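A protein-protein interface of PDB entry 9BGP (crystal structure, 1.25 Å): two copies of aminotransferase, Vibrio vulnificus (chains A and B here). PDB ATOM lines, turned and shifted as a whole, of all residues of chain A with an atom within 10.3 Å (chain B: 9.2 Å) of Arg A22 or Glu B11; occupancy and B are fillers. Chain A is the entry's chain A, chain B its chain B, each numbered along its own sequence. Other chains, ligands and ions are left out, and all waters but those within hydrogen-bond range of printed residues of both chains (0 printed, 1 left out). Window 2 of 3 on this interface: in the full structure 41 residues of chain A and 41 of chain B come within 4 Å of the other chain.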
ATOM      1  N   ALA A  13     -28.651 -15.788 -15.451  1.00  0.00           N
ATOM      2  CA  ALA A  13     -28.969 -14.413 -15.803  1.00  0.00           C
ATOM      3  C   ALA A  13     -27.696 -13.577 -15.868  1.00  0.00           C
ATOM      4  O   ALA A  13     -27.544 -12.749 -16.762  1.00  0.00           O
ATOM      5  CB  ALA A  13     -29.949 -13.853 -14.812  1.00  0.00           C
ATOM      6  N   ILE A  14     -26.774 -13.832 -14.936  1.00  0.00           N
ATOM      7  CA  ILE A  14     -25.498 -13.129 -14.939  1.00  0.00           C
ATOM      8  C   ILE A  14     -24.744 -13.449 -16.229  1.00  0.00           C
ATOM      9  O   ILE A  14     -24.160 -12.561 -16.853  1.00  0.00           O
ATOM     10  CB  ILE A  14     -24.688 -13.440 -13.662  1.00  0.00           C
ATOM     11  CG1 ILE A  14     -25.419 -12.967 -12.403  1.00  0.00           C
ATOM     12  CG2 ILE A  14     -23.289 -12.851 -13.740  1.00  0.00           C
ATOM     13  CD1 ILE A  14     -24.736 -13.347 -11.102  1.00  0.00           C
ATOM     14  N   GLU A  15     -24.774 -14.722 -16.655  1.00  0.00           N
ATOM     15  CA  GLU A  15     -24.123 -15.123 -17.889  1.00  0.00           C
ATOM     16  C   GLU A  15     -24.792 -14.454 -19.093  1.00  0.00           C
ATOM     17  O   GLU A  15     -24.138 -14.065 -20.065  1.00  0.00           O
ATOM     18  CB  GLU A  15     -24.208 -16.645 -18.079  1.00  0.00           C
ATOM     19  CG  GLU A  15     -23.653 -17.466 -16.934  1.00  0.00           C
ATOM     20  CD  GLU A  15     -23.610 -18.968 -17.174  1.00  0.00           C
ATOM     21  OE1 GLU A  15     -23.861 -19.399 -18.328  1.00  0.00           O
ATOM     22  OE2 GLU A  15     -23.332 -19.709 -16.199  1.00  0.00           O
ATOM     23  N   LYS A  16     -26.115 -14.330 -19.050  1.00  0.00           N
ATOM     24  CA  LYS A  16     -26.832 -13.692 -20.136  1.00  0.00           C
ATOM     25  C   LYS A  16     -26.459 -12.213 -20.201  1.00  0.00           C
ATOM     26  O   LYS A  16     -26.224 -11.690 -21.283  1.00  0.00           O
ATOM     27  CB  LYS A  16     -28.342 -13.889 -19.987  1.00  0.00           C
ATOM     28  CG  LYS A  16     -29.187 -13.211 -21.056  1.00  0.00           C
ATOM     29  CD  LYS A  16     -29.017 -13.803 -22.447  1.00  0.00           C
ATOM     30  CE  LYS A  16     -29.677 -15.159 -22.600  1.00  0.00           C
ATOM     31  NZ  LYS A  16     -31.153 -15.084 -22.431  1.00  0.00           N
ATOM     32  N   VAL A  17     -26.371 -11.561 -19.043  1.00  0.00           N
ATOM     33  CA  VAL A  17     -25.910 -10.173 -19.006  1.00  0.00           C
ATOM     34  C   VAL A  17     -24.521 -10.028 -19.641  1.00  0.00           C
ATOM     35  O   VAL A  17     -24.291  -9.144 -20.464  1.00  0.00           O
ATOM     36  CB  VAL A  17     -25.921  -9.575 -17.584  1.00  0.00           C
ATOM     37  CG1 VAL A  17     -25.190  -8.245 -17.521  1.00  0.00           C
ATOM     38  CG2 VAL A  17     -27.331  -9.417 -17.050  1.00  0.00           C
ATOM     39  N   ALA A  18     -23.595 -10.920 -19.249  1.00  0.00           N
ATOM     40  CA  ALA A  18     -22.249 -10.903 -19.817  1.00  0.00           C
ATOM     41  C   ALA A  18     -22.281 -11.072 -21.336  1.00  0.00           C
ATOM     42  O   ALA A  18     -21.595 -10.349 -22.057  1.00  0.00           O
ATOM     43  CB  ALA A  18     -21.401 -11.952 -19.147  1.00  0.00           C
ATOM     44  N   ASP A  19     -23.123 -11.988 -21.823  1.00  0.00           N
ATOM     45  CA  ASP A  19     -23.255 -12.220 -23.254  1.00  0.00           C
ATOM     46  C   ASP A  19     -23.760 -10.966 -23.953  1.00  0.00           C
ATOM     47  O   ASP A  19     -23.289 -10.620 -25.031  1.00  0.00           O
ATOM     48  CB  ASP A  19     -24.219 -13.358 -23.590  1.00  0.00           C
ATOM     49  CG  ASP A  19     -23.737 -14.758 -23.253  1.00  0.00           C
ATOM     50  OD1 ASP A  19     -22.529 -14.935 -23.040  1.00  0.00           O
ATOM     51  OD2 ASP A  19     -24.607 -15.648 -23.168  1.00  0.00           O
ATOM     52  N   ILE A  20     -24.753 -10.283 -23.351  1.00  0.00           N
ATOM     53  CA  ILE A  20     -25.294  -9.067 -23.937  1.00  0.00           C
ATOM     54  C   ILE A  20     -24.223  -7.983 -24.004  1.00  0.00           C
ATOM     55  O   ILE A  20     -24.081  -7.291 -25.014  1.00  0.00           O
ATOM     56  CB  ILE A  20     -26.559  -8.613 -23.161  1.00  0.00           C
ATOM     57  CG1 ILE A  20     -27.734  -9.572 -23.381  1.00  0.00           C
ATOM     58  CG2 ILE A  20     -26.940  -7.188 -23.538  1.00  0.00           C
ATOM     59  CD1 ILE A  20     -28.861  -9.455 -22.372  1.00  0.00           C
ATOM     60  N   LEU A  21     -23.501  -7.777 -22.901  1.00  0.00           N
ATOM     61  CA  LEU A  21     -22.457  -6.759 -22.891  1.00  0.00           C
ATOM     62  C   LEU A  21     -21.393  -7.049 -23.945  1.00  0.00           C
ATOM     63  O   LEU A  21     -20.841  -6.109 -24.507  1.00  0.00           O
ATOM     64  CB  LEU A  21     -21.821  -6.667 -21.499  1.00  0.00           C
ATOM     65  CG  LEU A  21     -22.757  -6.243 -20.366  1.00  0.00           C
ATOM     66  CD1 LEU A  21     -21.996  -6.129 -19.073  1.00  0.00           C
ATOM     67  CD2 LEU A  21     -23.463  -4.934 -20.685  1.00  0.00           C
ATOM     68  N   ARG A  22     -21.088  -8.336 -24.159  1.00  0.00           N
ATOM     69  CA  ARG A  22     -19.947  -8.725 -24.983  1.00  0.00           C
ATOM     70  C   ARG A  22     -20.322  -8.584 -26.452  1.00  0.00           C
ATOM     71  O   ARG A  22     -19.495  -8.166 -27.264  1.00  0.00           O
ATOM     72  CB  ARG A  22     -19.534 -10.168 -24.644  1.00  0.00           C
ATOM     73  CG  ARG A  22     -18.233 -10.664 -25.273  1.00  0.00           C
ATOM     74  CD  ARG A  22     -17.817 -12.009 -24.681  1.00  0.00           C
ATOM     75  NE  ARG A  22     -17.453 -11.946 -23.260  1.00  0.00           N
ATOM     76  CZ  ARG A  22     -18.106 -12.535 -22.257  1.00  0.00           C
ATOM     77  NH1 ARG A  22     -17.652 -12.435 -21.021  1.00  0.00           N
ATOM     78  NH2 ARG A  22     -19.208 -13.227 -22.487  1.00  0.00           N
ATOM     79  N   GLY A  23     -21.556  -8.951 -26.793  1.00  0.00           N
ATOM     80  CA  GLY A  23     -21.903  -9.100 -28.194  1.00  0.00           C
ATOM     81  C   GLY A  23     -23.378  -8.922 -28.520  1.00  0.00           C
ATOM     82  O   GLY A  23     -23.804  -9.321 -29.606  1.00  0.00           O
ATOM     83  N   GLY A  24     -24.151  -8.323 -27.603  1.00  0.00           N
ATOM     84  CA  GLY A  24     -25.590  -8.197 -27.771  1.00  0.00           C
ATOM     85  C   GLY A  24     -26.070  -6.748 -27.870  1.00  0.00           C
ATOM     86  O   GLY A  24     -25.284  -5.811 -27.971  1.00  0.00           O
ATOM     87  N   GLN A  25     -27.386  -6.561 -27.902  1.00  0.00           N
ATOM     88  CA  GLN A  25     -27.976  -5.236 -27.959  1.00  0.00           C
ATOM     89  C   GLN A  25     -28.087  -4.726 -26.521  1.00  0.00           C
ATOM     90  O   GLN A  25     -28.579  -5.454 -25.662  1.00  0.00           O
ATOM     91  CB  GLN A  25     -29.350  -5.295 -28.635  1.00  0.00           C
ATOM     92  CG  GLN A  25     -30.027  -3.941 -28.725  1.00  0.00           C
ATOM     93  CD  GLN A  25     -31.270  -3.970 -29.568  1.00  0.00           C
ATOM     94  OE1 GLN A  25     -31.255  -4.386 -30.728  1.00  0.00           O
ATOM     95  NE2 GLN A  25     -32.361  -3.488 -29.005  1.00  0.00           N
ATOM     96  N   LEU A  26     -27.607  -3.507 -26.271  1.00  0.00           N
ATOM     97  CA  LEU A  26     -27.593  -2.951 -24.921  1.00  0.00           C
ATOM     98  C   LEU A  26     -28.903  -2.237 -24.617  1.00  0.00           C
ATOM     99  O   LEU A  26     -29.409  -2.379 -23.499  1.00  0.00           O
ATOM    100  CB  LEU A  26     -26.427  -1.969 -24.793  1.00  0.00           C
ATOM    101  CG  LEU A  26     -25.048  -2.560 -25.083  1.00  0.00           C
ATOM    102  CD1 LEU A  26     -23.951  -1.519 -24.858  1.00  0.00           C
ATOM    103  CD2 LEU A  26     -24.744  -3.783 -24.233  1.00  0.00           C
ATOM    104  N   ASN A 234     -31.509  -3.539 -22.112  1.00  0.00           N
ATOM    105  CA  ASN A 234     -31.810  -4.924 -22.437  1.00  0.00           C
ATOM    106  C   ASN A 234     -31.207  -5.864 -21.399  1.00  0.00           C
ATOM    107  O   ASN A 234     -31.809  -6.907 -21.118  1.00  0.00           O
ATOM    108  CB  ASN A 234     -31.277  -5.206 -23.843  1.00  0.00           C
ATOM    109  CG  ASN A 234     -31.839  -6.465 -24.462  1.00  0.00           C
ATOM    110  OD1 ASN A 234     -33.043  -6.710 -24.419  1.00  0.00           O
ATOM    111  ND2 ASN A 234     -30.965  -7.232 -25.086  1.00  0.00           N
ATOM    112  N   PHE A 235     -30.040  -5.539 -20.838  1.00  0.00           N
ATOM    113  CA  PHE A 235     -29.431  -6.419 -19.847  1.00  0.00           C
ATOM    114  C   PHE A 235     -30.168  -6.330 -18.516  1.00  0.00           C
ATOM    115  O   PHE A 235     -30.273  -7.338 -17.825  1.00  0.00           O
ATOM    116  CB  PHE A 235     -27.917  -6.243 -19.703  1.00  0.00           C
ATOM    117  CG  PHE A 235     -27.413  -4.825 -19.538  1.00  0.00           C
ATOM    118  CD1 PHE A 235     -27.140  -4.012 -20.642  1.00  0.00           C
ATOM    119  CD2 PHE A 235     -27.143  -4.333 -18.271  1.00  0.00           C
ATOM    120  CE1 PHE A 235     -26.648  -2.730 -20.469  1.00  0.00           C
ATOM    121  CE2 PHE A 235     -26.655  -3.051 -18.104  1.00  0.00           C
ATOM    122  CZ  PHE A 235     -26.416  -2.256 -19.205  1.00  0.00           C
ATOM    123  N   GLN B   6     -20.387   0.174 -32.505  1.00  0.00           N
ATOM    124  CA  GLN B   6     -20.322  -1.166 -31.963  1.00  0.00           C
ATOM    125  C   GLN B   6     -19.426  -1.131 -30.730  1.00  0.00           C
ATOM    126  O   GLN B   6     -18.301  -1.599 -30.758  1.00  0.00           O
ATOM    127  CB  GLN B   6     -19.764  -2.123 -33.022  1.00  0.00           C
ATOM    128  CG  GLN B   6     -19.588  -3.546 -32.525  1.00  0.00           C
ATOM    129  CD  GLN B   6     -20.936  -4.083 -32.128  1.00  0.00           C
ATOM    130  OE1 GLN B   6     -21.316  -4.042 -30.960  1.00  0.00           O
ATOM    131  NE2 GLN B   6     -21.689  -4.531 -33.121  1.00  0.00           N
ATOM    132  N   PRO B   7     -19.866  -0.517 -29.613  1.00  0.00           N
ATOM    133  CA  PRO B   7     -18.977  -0.299 -28.479  1.00  0.00           C
ATOM    134  C   PRO B   7     -18.519  -1.628 -27.899  1.00  0.00           C
ATOM    135  O   PRO B   7     -19.324  -2.537 -27.732  1.00  0.00           O
ATOM    136  CB  PRO B   7     -19.806   0.518 -27.475  1.00  0.00           C
ATOM    137  CG  PRO B   7     -21.243   0.358 -27.926  1.00  0.00           C
ATOM    138  CD  PRO B   7     -21.215   0.007 -29.404  1.00  0.00           C
ATOM    139  N   GLN B   8     -17.217  -1.718 -27.612  1.00  0.00           N
ATOM    140  CA  GLN B   8     -16.622  -2.897 -27.017  1.00  0.00           C
ATOM    141  C   GLN B   8     -16.336  -2.578 -25.554  1.00  0.00           C
ATOM    142  O   GLN B   8     -15.452  -1.799 -25.212  1.00  0.00           O
ATOM    143  CB  GLN B   8     -15.385  -3.330 -27.802  1.00  0.00           C
ATOM    144  CG  GLN B   8     -15.720  -3.802 -29.209  1.00  0.00           C
ATOM    145  CD  GLN B   8     -14.501  -4.221 -29.985  1.00  0.00           C
ATOM    146  OE1 GLN B   8     -14.321  -5.397 -30.308  1.00  0.00           O
ATOM    147  NE2 GLN B   8     -13.656  -3.251 -30.298  1.00  0.00           N
ATOM    148  N   ILE B   9     -17.090  -3.240 -24.696  1.00  0.00           N
ATOM    149  CA  ILE B   9     -16.945  -3.080 -23.273  1.00  0.00           C
ATOM    150  C   ILE B   9     -15.816  -4.004 -22.847  1.00  0.00           C
ATOM    151  O   ILE B   9     -15.862  -5.197 -23.152  1.00  0.00           O
ATOM    152  CB  ILE B   9     -18.282  -3.430 -22.602  1.00  0.00           C
ATOM    153  CG1 ILE B   9     -19.376  -2.431 -22.983  1.00  0.00           C
ATOM    154  CG2 ILE B   9     -18.114  -3.538 -21.099  1.00  0.00           C
ATOM    155  CD1 ILE B   9     -20.759  -2.906 -22.584  1.00  0.00           C
ATOM    156  N   PRO B  10     -14.774  -3.494 -22.161  1.00  0.00           N
ATOM    157  CA  PRO B  10     -13.647  -4.333 -21.759  1.00  0.00           C
ATOM    158  C   PRO B  10     -14.121  -5.555 -20.983  1.00  0.00           C
ATOM    159  O   PRO B  10     -15.039  -5.509 -20.163  1.00  0.00           O
ATOM    160  CB  PRO B  10     -12.754  -3.412 -20.901  1.00  0.00           C
ATOM    161  CG  PRO B  10     -13.157  -2.006 -21.324  1.00  0.00           C
ATOM    162  CD  PRO B  10     -14.623  -2.098 -21.720  1.00  0.00           C
ATOM    163  N   GLU B  11     -13.439  -6.672 -21.211  1.00  0.00           N
ATOM    164  CA  GLU B  11     -13.769  -7.905 -20.524  1.00  0.00           C
ATOM    165  C   GLU B  11     -13.659  -7.719 -19.006  1.00  0.00           C
ATOM    166  O   GLU B  11     -14.467  -8.272 -18.254  1.00  0.00           O
ATOM    167  CB  GLU B  11     -12.858  -9.006 -21.089  1.00  0.00           C
ATOM    168  CG  GLU B  11     -13.303 -10.398 -20.743  1.00  0.00           C
ATOM    169  CD  GLU B  11     -14.722 -10.755 -21.167  1.00  0.00           C
ATOM    170  OE1 GLU B  11     -15.363 -11.485 -20.409  1.00  0.00           O
ATOM    171  OE2 GLU B  11     -15.157 -10.337 -22.257  1.00  0.00           O
ATOM    172  N   PHE B  12     -12.657  -6.979 -18.514  1.00  0.00           N
ATOM    173  CA  PHE B  12     -12.501  -6.817 -17.076  1.00  0.00           C
ATOM    174  C   PHE B  12     -13.737  -6.127 -16.486  1.00  0.00           C
ATOM    175  O   PHE B  12     -14.082  -6.397 -15.338  1.00  0.00           O
ATOM    176  CB  PHE B  12     -11.181  -6.114 -16.741  1.00  0.00           C
ATOM    177  CG  PHE B  12     -11.168  -4.618 -16.915  1.00  0.00           C
ATOM    178  CD1 PHE B  12     -11.572  -3.785 -15.879  1.00  0.00           C
ATOM    179  CD2 PHE B  12     -10.747  -4.042 -18.104  1.00  0.00           C
ATOM    180  CE1 PHE B  12     -11.556  -2.405 -16.035  1.00  0.00           C
ATOM    181  CE2 PHE B  12     -10.733  -2.665 -18.256  1.00  0.00           C
ATOM    182  CZ  PHE B  12     -11.126  -1.853 -17.217  1.00  0.00           C
ATOM    183  N   ALA B  13     -14.372  -5.258 -17.278  1.00  0.00           N
ATOM    184  CA  ALA B  13     -15.601  -4.577 -16.887  1.00  0.00           C
ATOM    185  C   ALA B  13     -16.776  -5.548 -16.805  1.00  0.00           C
ATOM    186  O   ALA B  13     -17.587  -5.465 -15.878  1.00  0.00           O
ATOM    187  CB  ALA B  13     -15.915  -3.466 -17.866  1.00  0.00           C
ATOM    188  N   ILE B  14     -16.876  -6.431 -17.801  1.00  0.00           N
ATOM    189  CA  ILE B  14     -17.907  -7.451 -17.805  1.00  0.00           C
ATOM    190  C   ILE B  14     -17.749  -8.305 -16.554  1.00  0.00           C
ATOM    191  O   ILE B  14     -18.721  -8.595 -15.870  1.00  0.00           O
ATOM    192  CB  ILE B  14     -17.885  -8.265 -19.114  1.00  0.00           C
ATOM    193  CG1 ILE B  14     -18.175  -7.378 -20.321  1.00  0.00           C
ATOM    194  CG2 ILE B  14     -18.868  -9.414 -19.031  1.00  0.00           C
ATOM    195  CD1 ILE B  14     -18.079  -8.072 -21.657  1.00  0.00           C
ATOM    196  N   GLU B  15     -16.512  -8.709 -16.216  1.00  0.00           N
ATOM    197  CA  GLU B  15     -16.281  -9.496 -15.012  1.00  0.00           C
ATOM    198  C   GLU B  15     -16.668  -8.703 -13.757  1.00  0.00           C
ATOM    199  O   GLU B  15     -17.231  -9.258 -12.825  1.00  0.00           O
ATOM    200  CB  GLU B  15     -14.807  -9.925 -14.937  1.00  0.00           C
ATOM    201  CG  GLU B  15     -14.295 -10.684 -16.154  1.00  0.00           C
ATOM    202  CD  GLU B  15     -12.779 -10.802 -16.255  1.00  0.00           C
ATOM    203  OE1 GLU B  15     -12.076 -10.422 -15.279  1.00  0.00           O
ATOM    204  OE2 GLU B  15     -12.295 -11.259 -17.322  1.00  0.00           O
ATOM    205  N   LYS B  16     -16.390  -7.401 -13.722  1.00  0.00           N
ATOM    206  CA  LYS B  16     -16.768  -6.593 -12.577  1.00  0.00           C
ATOM    207  C   LYS B  16     -18.288  -6.513 -12.442  1.00  0.00           C
ATOM    208  O   LYS B  16     -18.816  -6.560 -11.345  1.00  0.00           O
ATOM    209  CB  LYS B  16     -16.210  -5.177 -12.705  1.00  0.00           C
ATOM    210  CG  LYS B  16     -16.502  -4.245 -11.534  1.00  0.00           C
ATOM    211  CD  LYS B  16     -16.015  -4.750 -10.179  1.00  0.00           C
ATOM    212  CE  LYS B  16     -16.394  -3.837  -9.029  1.00  0.00           C
ATOM    213  NZ  LYS B  16     -16.134  -4.455  -7.704  1.00  0.00           N
ATOM    214  N   VAL B  17     -18.982  -6.333 -13.566  1.00  0.00           N
ATOM    215  CA  VAL B  17     -20.433  -6.335 -13.549  1.00  0.00           C
ATOM    216  C   VAL B  17     -20.941  -7.659 -12.973  1.00  0.00           C
ATOM    217  O   VAL B  17     -21.838  -7.681 -12.135  1.00  0.00           O
ATOM    218  CB  VAL B  17     -21.027  -6.103 -14.947  1.00  0.00           C
ATOM    219  CG1 VAL B  17     -22.519  -6.418 -14.984  1.00  0.00           C
ATOM    220  CG2 VAL B  17     -20.750  -4.687 -15.448  1.00  0.00           C
ATOM    221  N   ALA B  18     -20.373  -8.779 -13.446  1.00  0.00           N
ATOM    222  CA  ALA B  18     -20.814 -10.078 -12.943  1.00  0.00           C
ATOM    223  C   ALA B  18     -20.598 -10.176 -11.432  1.00  0.00           C
ATOM    224  O   ALA B  18     -21.455 -10.647 -10.695  1.00  0.00           O
ATOM    225  CB  ALA B  18     -20.050 -11.169 -13.658  1.00  0.00           C
ATOM    226  N   ASP B  19     -19.439  -9.717 -10.963  1.00  0.00           N
ATOM    227  CA  ASP B  19     -19.125  -9.718  -9.541  1.00  0.00           C
ATOM    228  C   ASP B  19     -20.152  -8.892  -8.770  1.00  0.00           C
ATOM    229  O   ASP B  19     -20.559  -9.254  -7.672  1.00  0.00           O
ATOM    230  CB  ASP B  19     -17.716  -9.173  -9.293  1.00  0.00           C
ATOM    231  CG  ASP B  19     -16.574 -10.094  -9.668  1.00  0.00           C
ATOM    232  OD1 ASP B  19     -16.819 -11.294  -9.864  1.00  0.00           O
ATOM    233  OD2 ASP B  19     -15.437  -9.579  -9.726  1.00  0.00           O
ATOM    234  N   ILE B 239     -19.195  -0.099 -15.832  1.00  0.00           N
ATOM    235  CA  ILE B 239     -18.928  -0.140 -17.257  1.00  0.00           C
ATOM    236  C   ILE B 239     -18.330   1.185 -17.697  1.00  0.00           C
ATOM    237  O   ILE B 239     -17.326   1.208 -18.397  1.00  0.00           O
ATOM    238  CB  ILE B 239     -20.215  -0.477 -18.039  1.00  0.00           C
ATOM    239  CG1 ILE B 239     -20.753  -1.870 -17.712  1.00  0.00           C
ATOM    240  CG2 ILE B 239     -19.973  -0.329 -19.522  1.00  0.00           C
ATOM    241  CD1 ILE B 239     -22.148  -2.125 -18.160  1.00  0.00           C
ATOM    242  N   ALA B 242     -14.764   1.894 -16.676  1.00  0.00           N
ATOM    243  CA  ALA B 242     -13.818   1.035 -17.359  1.00  0.00           C
ATOM    244  C   ALA B 242     -13.469   1.576 -18.740  1.00  0.00           C
ATOM    245  O   ALA B 242     -12.353   1.364 -19.225  1.00  0.00           O
ATOM    246  CB  ALA B 242     -14.370  -0.369 -17.484  1.00  0.00           C
ATOM    247  N   ILE B 243     -14.406   2.278 -19.382  1.00  0.00           N
ATOM    248  CA  ILE B 243     -14.211   2.737 -20.748  1.00  0.00           C
ATOM    249  C   ILE B 243     -13.516   4.101 -20.766  1.00  0.00           C
ATOM    250  O   ILE B 243     -12.760   4.414 -21.686  1.00  0.00           O
ATOM    251  CB  ILE B 243     -15.543   2.793 -21.517  1.00  0.00           C
ATOM    252  CG1 ILE B 243     -16.098   1.378 -21.723  1.00  0.00           C
ATOM    253  CG2 ILE B 243     -15.387   3.540 -22.832  1.00  0.00           C
ATOM    254  CD1 ILE B 243     -17.534   1.346 -22.233  1.00  0.00           C
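The side-chain carboxylate (OE1) of Glu B11 is in salt-bridge range of the guanidinium group (NH1) of Arg A22, at 2.6 Å.
The side-chain carboxylate (OD1) of Asp A19 is in salt-bridge range of the guanidinium group (NH2) of Arg A22 (3.8 Å).
Ile A14 touches Ala B18 (CG2 to CB, 3.7 Å).
CB of Ala A18 touches CG2 of Ile B14, 3.6 Å away.
Ile B9 touches Leu A21 (CD1 to O, 3.7 Å).
Leu A21 touches Ile B14 (CB to CG1, 3.9 Å).
CD1 of Ile B239 touches CD2 of Leu A21, 3.999 Å away.
Arg A22 touches Ile B14 (NH1 to CG2, 3.8 Å).
Arg A22 touches just these residues of chain B: Glu B11 (2.6 Å) and Ile B14 (3.8 Å).
Of chain A, only Arg A22 comes within 4 Å of Glu B11.
No residue of chain B comes within 4 Å of Gly A23.
No residue of chain A comes within 4 Å of Ala B13.
No residue of chain A comes within 4 Å of Glu B15.
Printed residues of chain B within 4 Å of Ile A14: Ala B18.
Printed residues of chain B within 4 Å of Ala A18: Ile B14.
Printed residues of chain B within 4 Å of Leu A21: Ile B9 (3.7 Å), Ile B14 (3.9 Å) and Ile B239 (3.999 Å).
Printed residues of chain A within 4 Å of Ala B18: Ile A14 (3.7 Å).
Of the printed residues of chain A, Ile B239 touches Leu A21.
The nearest printed residue of chain B that does not touch Arg A22 is Pro B7 (5.7 Å).
The nearest residue of chain A that does not touch Glu B11 is Ala A18 (6.2 Å).
Of the 16 printed residues of chain A, 4 touch a printed residue of chain B.
Of the 17 printed residues of chain B, 5 touch a printed residue of chain A.
Printed residues of chain B that touch a printed residue of chain A: Ile B9, Glu B11, Ile B14, Ala B18 and Ile B239.
Hydrophobic or aromatic side chains of chain B within 4 Å of the printed part of chain A: Ile B9, Ile B14, Ala B18 and Ile B239.
Among the printed residues, Asp or Glu carboxylates within 4 Å of a Lys or Arg side-chain nitrogen of the other chain: Arg A22 with Glu B11.
Ile A14 touches Ala B18, and with the chains exchanged Ala A18 touches Ile B14.
7 positions are printed for both chains.
Of the 7 pairs that touch across the chains among the printed residues, 2 have their exchanged pair printed and touching as well.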
